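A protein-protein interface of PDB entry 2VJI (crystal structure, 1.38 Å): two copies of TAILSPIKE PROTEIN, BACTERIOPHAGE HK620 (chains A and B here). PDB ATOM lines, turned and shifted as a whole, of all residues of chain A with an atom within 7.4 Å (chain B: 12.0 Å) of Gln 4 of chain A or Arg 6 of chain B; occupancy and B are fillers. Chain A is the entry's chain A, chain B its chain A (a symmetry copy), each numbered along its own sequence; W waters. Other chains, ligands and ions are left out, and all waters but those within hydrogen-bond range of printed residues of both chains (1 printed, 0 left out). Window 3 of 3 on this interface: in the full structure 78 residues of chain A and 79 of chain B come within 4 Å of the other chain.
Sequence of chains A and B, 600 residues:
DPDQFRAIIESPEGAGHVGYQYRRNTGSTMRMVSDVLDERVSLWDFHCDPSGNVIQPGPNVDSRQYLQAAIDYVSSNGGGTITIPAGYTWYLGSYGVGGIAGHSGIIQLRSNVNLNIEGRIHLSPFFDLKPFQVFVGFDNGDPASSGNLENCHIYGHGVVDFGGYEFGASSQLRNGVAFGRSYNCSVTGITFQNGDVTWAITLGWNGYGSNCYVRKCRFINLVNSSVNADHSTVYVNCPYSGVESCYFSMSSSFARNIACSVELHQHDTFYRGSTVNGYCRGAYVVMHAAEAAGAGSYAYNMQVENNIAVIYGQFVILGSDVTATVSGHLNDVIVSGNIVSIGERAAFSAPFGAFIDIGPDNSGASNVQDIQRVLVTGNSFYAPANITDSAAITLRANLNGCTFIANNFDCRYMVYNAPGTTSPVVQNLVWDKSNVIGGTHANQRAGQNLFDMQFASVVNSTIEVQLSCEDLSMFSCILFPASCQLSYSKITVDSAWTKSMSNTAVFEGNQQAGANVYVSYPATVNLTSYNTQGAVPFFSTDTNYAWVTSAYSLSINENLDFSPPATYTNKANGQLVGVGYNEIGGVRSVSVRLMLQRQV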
ATOM      1  N   ASP A   3       0.350 -32.076  -1.362  1.00  0.00           N
ATOM      2  CA  ASP A   3       1.476 -31.206  -1.812  1.00  0.00           C
ATOM      3  C   ASP A   3       2.386 -31.948  -2.787  1.00  0.00           C
ATOM      4  O   ASP A   3       3.243 -32.730  -2.367  1.00  0.00           O
ATOM      5  N   GLN A   4       2.193 -31.694  -4.082  1.00  0.00           N
ATOM      6  CA  GLN A   4       2.978 -32.336  -5.138  1.00  0.00           C
ATOM      7  C   GLN A   4       4.471 -32.036  -5.010  1.00  0.00           C
ATOM      8  O   GLN A   4       5.301 -32.946  -5.094  1.00  0.00           O
ATOM      9  CB  GLN A   4       2.502 -31.883  -6.522  1.00  0.00           C
ATOM     10  CG  GLN A   4       3.269 -32.531  -7.677  1.00  0.00           C
ATOM     11  CD  GLN A   4       3.038 -31.842  -9.009  1.00  0.00           C
ATOM     12  OE1 GLN A   4       1.949 -31.336  -9.285  1.00  0.00           O
ATOM     13  NE2 GLN A   4       4.070 -31.826  -9.847  1.00  0.00           N
ATOM     14  N   PHE A   5       4.816 -30.764  -4.831  1.00  0.00           N
ATOM     15  CA  PHE A   5       6.226 -30.382  -4.709  1.00  0.00           C
ATOM     16  C   PHE A   5       6.873 -31.035  -3.492  1.00  0.00           C
ATOM     17  O   PHE A   5       8.010 -31.504  -3.577  1.00  0.00           O
ATOM     18  CB  PHE A   5       6.391 -28.865  -4.669  1.00  0.00           C
ATOM     19  CG  PHE A   5       7.822 -28.415  -4.685  1.00  0.00           C
ATOM     20  CD1 PHE A   5       8.646 -28.743  -5.753  1.00  0.00           C
ATOM     21  CD2 PHE A   5       8.342 -27.652  -3.653  1.00  0.00           C
ATOM     22  CE1 PHE A   5       9.972 -28.334  -5.783  1.00  0.00           C
ATOM     23  CE2 PHE A   5       9.660 -27.232  -3.680  1.00  0.00           C
ATOM     24  CZ  PHE A   5      10.476 -27.574  -4.747  1.00  0.00           C
ATOM     25  N   ARG A   6       6.150 -31.084  -2.374  1.00  0.00           N
ATOM     26  CA  ARG A   6       6.651 -31.744  -1.166  1.00  0.00           C
ATOM     27  C   ARG A   6       6.992 -33.197  -1.489  1.00  0.00           C
ATOM     28  O   ARG A   6       8.061 -33.676  -1.131  1.00  0.00           O
ATOM     29  CB  ARG A   6       5.621 -31.703  -0.028  1.00  0.00           C
ATOM     30  CG  ARG A   6       6.035 -32.497   1.227  1.00  0.00           C
ATOM     31  CD  ARG A   6       4.908 -32.608   2.259  1.00  0.00           C
ATOM     32  NE  ARG A   6       4.725 -31.405   3.078  1.00  0.00           N
ATOM     33  CZ  ARG A   6       5.229 -31.218   4.302  1.00  0.00           C
ATOM     34  NH1 ARG A   6       5.976 -32.149   4.896  1.00  0.00           N
ATOM     35  NH2 ARG A   6       4.985 -30.080   4.944  1.00  0.00           N
ATOM     36  N   ALA A   7       6.068 -33.890  -2.151  1.00  0.00           N
ATOM     37  CA  ALA A   7       6.266 -35.292  -2.523  1.00  0.00           C
ATOM     38  C   ALA A   7       7.522 -35.491  -3.363  1.00  0.00           C
ATOM     39  O   ALA A   7       8.276 -36.438  -3.141  1.00  0.00           O
ATOM     40  CB  ALA A   7       5.047 -35.821  -3.266  1.00  0.00           C
ATOM     41  N   ILE A   8       7.754 -34.590  -4.312  1.00  0.00           N
ATOM     42  CA  ILE A   8       8.931 -34.677  -5.173  1.00  0.00           C
ATOM     43  C   ILE A   8      10.203 -34.466  -4.369  1.00  0.00           C
ATOM     44  O   ILE A   8      11.162 -35.221  -4.492  1.00  0.00           O
ATOM     45  CB  ILE A   8       8.863 -33.654  -6.329  1.00  0.00           C
ATOM     46  CG1 ILE A   8       7.738 -34.043  -7.294  1.00  0.00           C
ATOM     47  CG2 ILE A   8      10.204 -33.581  -7.071  1.00  0.00           C
ATOM     48  CD1 ILE A   8       7.446 -33.015  -8.364  1.00  0.00           C
ATOM     49  N   ILE A   9      10.202 -33.448  -3.520  1.00  0.00           N
ATOM     50  CA  ILE A   9      11.391 -33.130  -2.733  1.00  0.00           C
ATOM     51  C   ILE A   9      11.729 -34.217  -1.716  1.00  0.00           C
ATOM     52  O   ILE A   9      12.900 -34.535  -1.491  1.00  0.00           O
ATOM     53  CB  ILE A   9      11.226 -31.754  -2.040  1.00  0.00           C
ATOM     54  CG1 ILE A   9      11.213 -30.634  -3.096  1.00  0.00           C
ATOM     55  CG2 ILE A   9      12.315 -31.512  -1.006  1.00  0.00           C
ATOM     56  CD1 ILE A   9      12.498 -30.508  -3.919  1.00  0.00           C
ATOM     57  N   GLU A  10      10.711 -34.799  -1.113  1.00  0.00           N
ATOM     58  CA  GLU A  10      10.920 -35.837  -0.116  1.00  0.00           C
ATOM     59  C   GLU A  10      11.225 -37.212  -0.732  1.00  0.00           C
ATOM     60  O   GLU A  10      11.719 -38.094  -0.039  1.00  0.00           O
ATOM     61  CB  GLU A  10       9.737 -35.860   0.856  1.00  0.00           C
ATOM     62  CG  GLU A  10       9.606 -34.536   1.637  1.00  0.00           C
ATOM     63  CD  GLU A  10       8.533 -34.556   2.709  1.00  0.00           C
ATOM     64  OE1 GLU A  10       7.638 -35.427   2.653  1.00  0.00           O
ATOM     65  OE2 GLU A  10       8.588 -33.685   3.612  1.00  0.00           O
ATOM     66  N   HIS A  17      16.098 -31.836  -7.755  1.00  0.00           N
ATOM     67  CA  HIS A  17      15.264 -30.659  -7.988  1.00  0.00           C
ATOM     68  C   HIS A  17      15.673 -29.453  -7.143  1.00  0.00           C
ATOM     69  O   HIS A  17      14.939 -28.468  -7.080  1.00  0.00           O
ATOM     70  CB  HIS A  17      13.798 -30.991  -7.744  1.00  0.00           C
ATOM     71  CG  HIS A  17      13.258 -32.023  -8.676  1.00  0.00           C
ATOM     72  ND1 HIS A  17      12.709 -31.705  -9.899  1.00  0.00           N
ATOM     73  CD2 HIS A  17      13.190 -33.368  -8.570  1.00  0.00           C
ATOM     74  CE1 HIS A  17      12.319 -32.813 -10.502  1.00  0.00           C
ATOM     75  NE2 HIS A  17      12.596 -33.837  -9.715  1.00  0.00           N
ATOM     76  N   ASP B   3       4.033 -21.508  -8.185  1.00  0.00           N
ATOM     77  CA  ASP B   3       4.677 -21.877  -6.891  1.00  0.00           C
ATOM     78  C   ASP B   3       5.994 -21.130  -6.702  1.00  0.00           C
ATOM     79  O   ASP B   3       7.022 -21.529  -7.253  1.00  0.00           O
ATOM     80  N   GLN B   4       5.951 -20.051  -5.919  1.00  0.00           N
ATOM     81  CA  GLN B   4       7.128 -19.223  -5.650  1.00  0.00           C
ATOM     82  C   GLN B   4       8.249 -20.015  -4.979  1.00  0.00           C
ATOM     83  O   GLN B   4       9.409 -19.930  -5.392  1.00  0.00           O
ATOM     84  CB  GLN B   4       6.763 -18.033  -4.757  1.00  0.00           C
ATOM     85  CG  GLN B   4       7.947 -17.111  -4.450  1.00  0.00           C
ATOM     86  CD  GLN B   4       7.672 -16.146  -3.313  1.00  0.00           C
ATOM     87  OE1 GLN B   4       6.547 -15.677  -3.130  1.00  0.00           O
ATOM     88  NE2 GLN B   4       8.712 -15.838  -2.543  1.00  0.00           N
ATOM     89  N   PHE B   5       7.912 -20.764  -3.932  1.00  0.00           N
ATOM     90  CA  PHE B   5       8.924 -21.550  -3.219  1.00  0.00           C
ATOM     91  C   PHE B   5       9.562 -22.592  -4.132  1.00  0.00           C
ATOM     92  O   PHE B   5      10.778 -22.784  -4.090  1.00  0.00           O
ATOM     93  CB  PHE B   5       8.343 -22.201  -1.967  1.00  0.00           C
ATOM     94  CG  PHE B   5       9.367 -22.902  -1.125  1.00  0.00           C
ATOM     95  CD1 PHE B   5      10.432 -22.194  -0.584  1.00  0.00           C
ATOM     96  CD2 PHE B   5       9.262 -24.256  -0.851  1.00  0.00           C
ATOM     97  CE1 PHE B   5      11.388 -22.828   0.199  1.00  0.00           C
ATOM     98  CE2 PHE B   5      10.204 -24.893  -0.063  1.00  0.00           C
ATOM     99  CZ  PHE B   5      11.269 -24.178   0.462  1.00  0.00           C
ATOM    100  N   ARG B   6       8.752 -23.244  -4.966  1.00  0.00           N
ATOM    101  CA  ARG B   6       9.268 -24.219  -5.929  1.00  0.00           C
ATOM    102  C   ARG B   6      10.307 -23.545  -6.822  1.00  0.00           C
ATOM    103  O   ARG B   6      11.387 -24.084  -7.030  1.00  0.00           O
ATOM    104  CB  ARG B   6       8.148 -24.803  -6.803  1.00  0.00           C
ATOM    105  CG  ARG B   6       8.643 -25.735  -7.925  1.00  0.00           C
ATOM    106  CD  ARG B   6       7.532 -26.136  -8.899  1.00  0.00           C
ATOM    107  NE  ARG B   6       6.653 -27.199  -8.401  1.00  0.00           N
ATOM    108  CZ  ARG B   6       6.769 -28.500  -8.691  1.00  0.00           C
ATOM    109  NH1 ARG B   6       7.740 -28.950  -9.486  1.00  0.00           N
ATOM    110  NH2 ARG B   6       5.902 -29.366  -8.177  1.00  0.00           N
ATOM    111  N   ALA B   7       9.962 -22.376  -7.357  1.00  0.00           N
ATOM    112  CA  ALA B   7      10.864 -21.624  -8.230  1.00  0.00           C
ATOM    113  C   ALA B   7      12.198 -21.322  -7.559  1.00  0.00           C
ATOM    114  O   ALA B   7      13.252 -21.454  -8.178  1.00  0.00           O
ATOM    115  CB  ALA B   7      10.203 -20.332  -8.690  1.00  0.00           C
ATOM    116  N   ILE B   8      12.151 -20.936  -6.286  1.00  0.00           N
ATOM    117  CA  ILE B   8      13.368 -20.627  -5.540  1.00  0.00           C
ATOM    118  C   ILE B   8      14.213 -21.875  -5.348  1.00  0.00           C
ATOM    119  O   ILE B   8      15.419 -21.864  -5.575  1.00  0.00           O
ATOM    120  CB  ILE B   8      13.044 -19.995  -4.167  1.00  0.00           C
ATOM    121  CG1 ILE B   8      12.438 -18.603  -4.373  1.00  0.00           C
ATOM    122  CG2 ILE B   8      14.303 -19.908  -3.297  1.00  0.00           C
ATOM    123  CD1 ILE B   8      11.903 -17.958  -3.114  1.00  0.00           C
ATOM    124  N   ILE B   9      13.573 -22.967  -4.952  1.00  0.00           N
ATOM    125  CA  ILE B   9      14.300 -24.207  -4.694  1.00  0.00           C
ATOM    126  C   ILE B   9      14.913 -24.802  -5.959  1.00  0.00           C
ATOM    127  O   ILE B   9      16.030 -25.327  -5.938  1.00  0.00           O
ATOM    128  CB  ILE B   9      13.378 -25.233  -3.988  1.00  0.00           C
ATOM    129  CG1 ILE B   9      13.037 -24.743  -2.570  1.00  0.00           C
ATOM    130  CG2 ILE B   9      14.009 -26.617  -3.946  1.00  0.00           C
ATOM    131  CD1 ILE B   9      14.240 -24.585  -1.635  1.00  0.00           C
ATOM    132  N   GLU B  10      14.197 -24.709  -7.063  1.00  0.00           N
ATOM    133  CA  GLU B  10      14.679 -25.255  -8.321  1.00  0.00           C
ATOM    134  C   GLU B  10      15.707 -24.347  -9.018  1.00  0.00           C
ATOM    135  O   GLU B  10      16.419 -24.802  -9.906  1.00  0.00           O
ATOM    136  CB  GLU B  10      13.489 -25.615  -9.213  1.00  0.00           C
ATOM    137  CG  GLU B  10      12.605 -26.711  -8.582  1.00  0.00           C
ATOM    138  CD  GLU B  10      11.489 -27.200  -9.485  1.00  0.00           C
ATOM    139  OE1 GLU B  10      11.139 -26.489 -10.453  1.00  0.00           O
ATOM    140  OE2 GLU B  10      10.957 -28.305  -9.217  1.00  0.00           O
ATOM    141  N   SER B  11      15.818 -23.092  -8.580  1.00  0.00           N
ATOM    142  CA  SER B  11      16.784 -22.145  -9.150  1.00  0.00           C
ATOM    143  C   SER B  11      18.183 -22.464  -8.623  1.00  0.00           C
ATOM    144  O   SER B  11      18.316 -23.222  -7.669  1.00  0.00           O
ATOM    145  CB  SER B  11      16.440 -20.716  -8.737  1.00  0.00           C
ATOM    146  OG  SER B  11      16.765 -20.501  -7.376  1.00  0.00           O
ATOM    147  N   PRO B  12      19.228 -21.871  -9.230  1.00  0.00           N
ATOM    148  CA  PRO B  12      20.585 -22.078  -8.724  1.00  0.00           C
ATOM    149  C   PRO B  12      20.807 -21.635  -7.268  1.00  0.00           C
ATOM    150  O   PRO B  12      21.817 -22.023  -6.671  1.00  0.00           O
ATOM    151  CB  PRO B  12      21.451 -21.252  -9.680  1.00  0.00           C
ATOM    152  CG  PRO B  12      20.641 -21.066 -10.879  1.00  0.00           C
ATOM    153  CD  PRO B  12      19.226 -21.033 -10.440  1.00  0.00           C
ATOM    154  N   GLU B  13      19.886 -20.848  -6.703  1.00  0.00           N
ATOM    155  CA  GLU B  13      19.988 -20.414  -5.303  1.00  0.00           C
ATOM    156  C   GLU B  13      19.257 -21.358  -4.345  1.00  0.00           C
ATOM    157  O   GLU B  13      19.246 -21.132  -3.143  1.00  0.00           O
ATOM    158  CB  GLU B  13      19.440 -18.989  -5.125  1.00  0.00           C
ATOM    159  CG  GLU B  13      20.246 -17.896  -5.831  1.00  0.00           C
ATOM    160  CD  GLU B  13      20.079 -17.895  -7.338  1.00  0.00           C
ATOM    161  OE1 GLU B  13      18.953 -18.135  -7.819  1.00  0.00           O
ATOM    162  OE2 GLU B  13      21.073 -17.630  -8.046  1.00  0.00           O
ATOM    163  N   GLY B  14      18.661 -22.423  -4.873  1.00  0.00           N
ATOM    164  CA  GLY B  14      17.867 -23.348  -4.075  1.00  0.00           C
ATOM    165  C   GLY B  14      18.545 -23.969  -2.876  1.00  0.00           C
ATOM    166  O   GLY B  14      17.976 -24.017  -1.777  1.00  0.00           O
ATOM    167  N   ALA B  15      19.770 -24.442  -3.071  1.00  0.00           N
ATOM    168  CA  ALA B  15      20.524 -25.065  -1.989  1.00  0.00           C
ATOM    169  C   ALA B  15      20.818 -24.074  -0.859  1.00  0.00           C
ATOM    170  O   ALA B  15      21.068 -24.477   0.271  1.00  0.00           O
ATOM    171  CB  ALA B  15      21.810 -25.662  -2.530  1.00  0.00           C
ATOM    172  N   GLY B  16      20.813 -22.781  -1.173  1.00  0.00           N
ATOM    173  CA  GLY B  16      21.004 -21.745  -0.171  1.00  0.00           C
ATOM    174  C   GLY B  16      19.779 -21.524   0.696  1.00  0.00           C
ATOM    175  O   GLY B  16      19.804 -20.684   1.601  1.00  0.00           O
ATOM    176  N   HIS B  17      18.688 -22.233   0.395  1.00  0.00           N
ATOM    177  CA  HIS B  17      17.458 -22.144   1.179  1.00  0.00           C
ATOM    178  C   HIS B  17      17.083 -23.459   1.863  1.00  0.00           C
ATOM    179  O   HIS B  17      15.974 -23.589   2.379  1.00  0.00           O
ATOM    180  CB  HIS B  17      16.305 -21.667   0.307  1.00  0.00           C
ATOM    181  CG  HIS B  17      16.501 -20.291  -0.238  1.00  0.00           C
ATOM    182  ND1 HIS B  17      16.108 -19.160   0.443  1.00  0.00           N
ATOM    183  CD2 HIS B  17      17.057 -19.864  -1.393  1.00  0.00           C
ATOM    184  CE1 HIS B  17      16.408 -18.093  -0.277  1.00  0.00           C
ATOM    185  NE2 HIS B  17      16.981 -18.494  -1.397  1.00  0.00           N
ATOM    186  N   VAL B  18      17.989 -24.432   1.863  1.00  0.00           N
ATOM    187  CA  VAL B  18      17.748 -25.704   2.536  1.00  0.00           C
ATOM    188  C   VAL B  18      18.698 -25.736   3.721  1.00  0.00           C
ATOM    189  O   VAL B  18      19.922 -25.692   3.550  1.00  0.00           O
ATOM    190  CB  VAL B  18      17.989 -26.925   1.619  1.00  0.00           C
ATOM    191  CG1 VAL B  18      17.680 -28.210   2.369  1.00  0.00           C
ATOM    192  CG2 VAL B  18      17.148 -26.830   0.355  1.00  0.00           C
HETATM  193  O   HOH W   1      13.392 -29.085 -11.251  1.00  0.00           O
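The side-chain amide nitrogen (NE2) of Gln 4 of chain A sits close to the guanidinium group (NH2) of Arg 6 of chain B (3.5 Å).
The side-chain carboxylate (OE2) of Glu 10 of chain B lies within salt-bridge range of the guanidinium group (NH1) of Arg 6 of chain B, at 3.3 Å.
CD1 of Phe 5 of chain A touches CZ of Arg 6 of chain B, at 3.5 Å.
CZ of Phe 5 of chain A touches CG2 of Ile 9 of chain B, at 3.7 Å.
CE1 of Phe 5 of chain A touches OE2 of Glu 10 of chain B (3.6 Å).
Ile 8 of chain A touches Arg 6 of chain B (CD1 to NH2, 3.97 Å).
His 17 of chain A touches Ile 9 of chain B.
O of His 17 of chain A touches CG of Glu 10 of chain B (3.3 Å).
Gln 4 of chain A touches just one residue of chain B: Arg 6.
Arg 6 of chain B touches just these residues of chain A: Gln 4 (3.5 Å), Phe 5 (3.5 Å) and Ile 8 (3.97 Å).
Of chain B, only Arg 6, Ile 9 and Glu 10 come within 4 Å of Phe 5 of chain A.
No residue of chain B comes within 4 Å of Ala 7 of chain A.
Printed residues of chain B within 4 Å of His 17 of chain A: Ile 9 (3.5 Å) and Glu 10 (3.3 Å).
Printed residues of chain A within 4 Å of Ile 9 of chain B: Phe 5 (3.7 Å) and His 17 (3.5 Å).
Of the printed residues of chain A, Glu 10 of chain B touches Phe 5 (3.6 Å) and His 17 (3.3 Å).
Glu 13 of chain B touches none of the printed residues of chain A.
Ala 15 of chain B touches none of the printed residues of chain A.
The nearest residue of chain B that does not touch Gln 4 of chain A is Glu 10 of chain B (7.8 Å).
The nearest residue of chain A that does not touch Arg 6 of chain B is His 17 of chain A (5.6 Å).
The nearest printed residue of chain A that does not touch Glu 10 of chain B is Ile 8 of chain A (5.7 Å).
Hydrophobic or aromatic side chains of chain B that line the printed part of chain A: Ile 9.
Printed residues of chain A that touch a printed residue of chain B: Gln 4, Phe 5, Ile 8 and His 17.
Hydrophobic or aromatic side chains of chain A that line the printed part of chain B: Phe 5, Ile 8 and His 17.
Among the printed residues, 7 pairs touch across the chains.
Among the printed residues, no Asp or Glu carboxylate lies within 4 Å of a Lys or Arg side-chain nitrogen of the other chain.
Phe 5 of chain A touches Ile 9 of chain B, but with the chains exchanged Ile 9 of chain A does not touch Phe 5 of chain B (6.6 Å).
Phe 5 of chain A touches Glu 10 of chain B, but with the chains exchanged Glu 10 of chain A does not touch Phe 5 of chain B (9.7 Å).
Ile 8 of chain A touches Arg 6 of chain B, but with the chains exchanged Arg 6 of chain A does not touch Ile 8 of chain B (12.4 Å).
His 17 of chain A touches Ile 9 of chain B, but with the chains exchanged Ile 9 of chain A does not touch His 17 of chain B (9.4 Å).
9 positions are printed for both chains.
Water W1 bridges ND1 of His 17 of chain A (3.0 Å) and OE2 of Glu 10 of chain B (3.3 Å).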
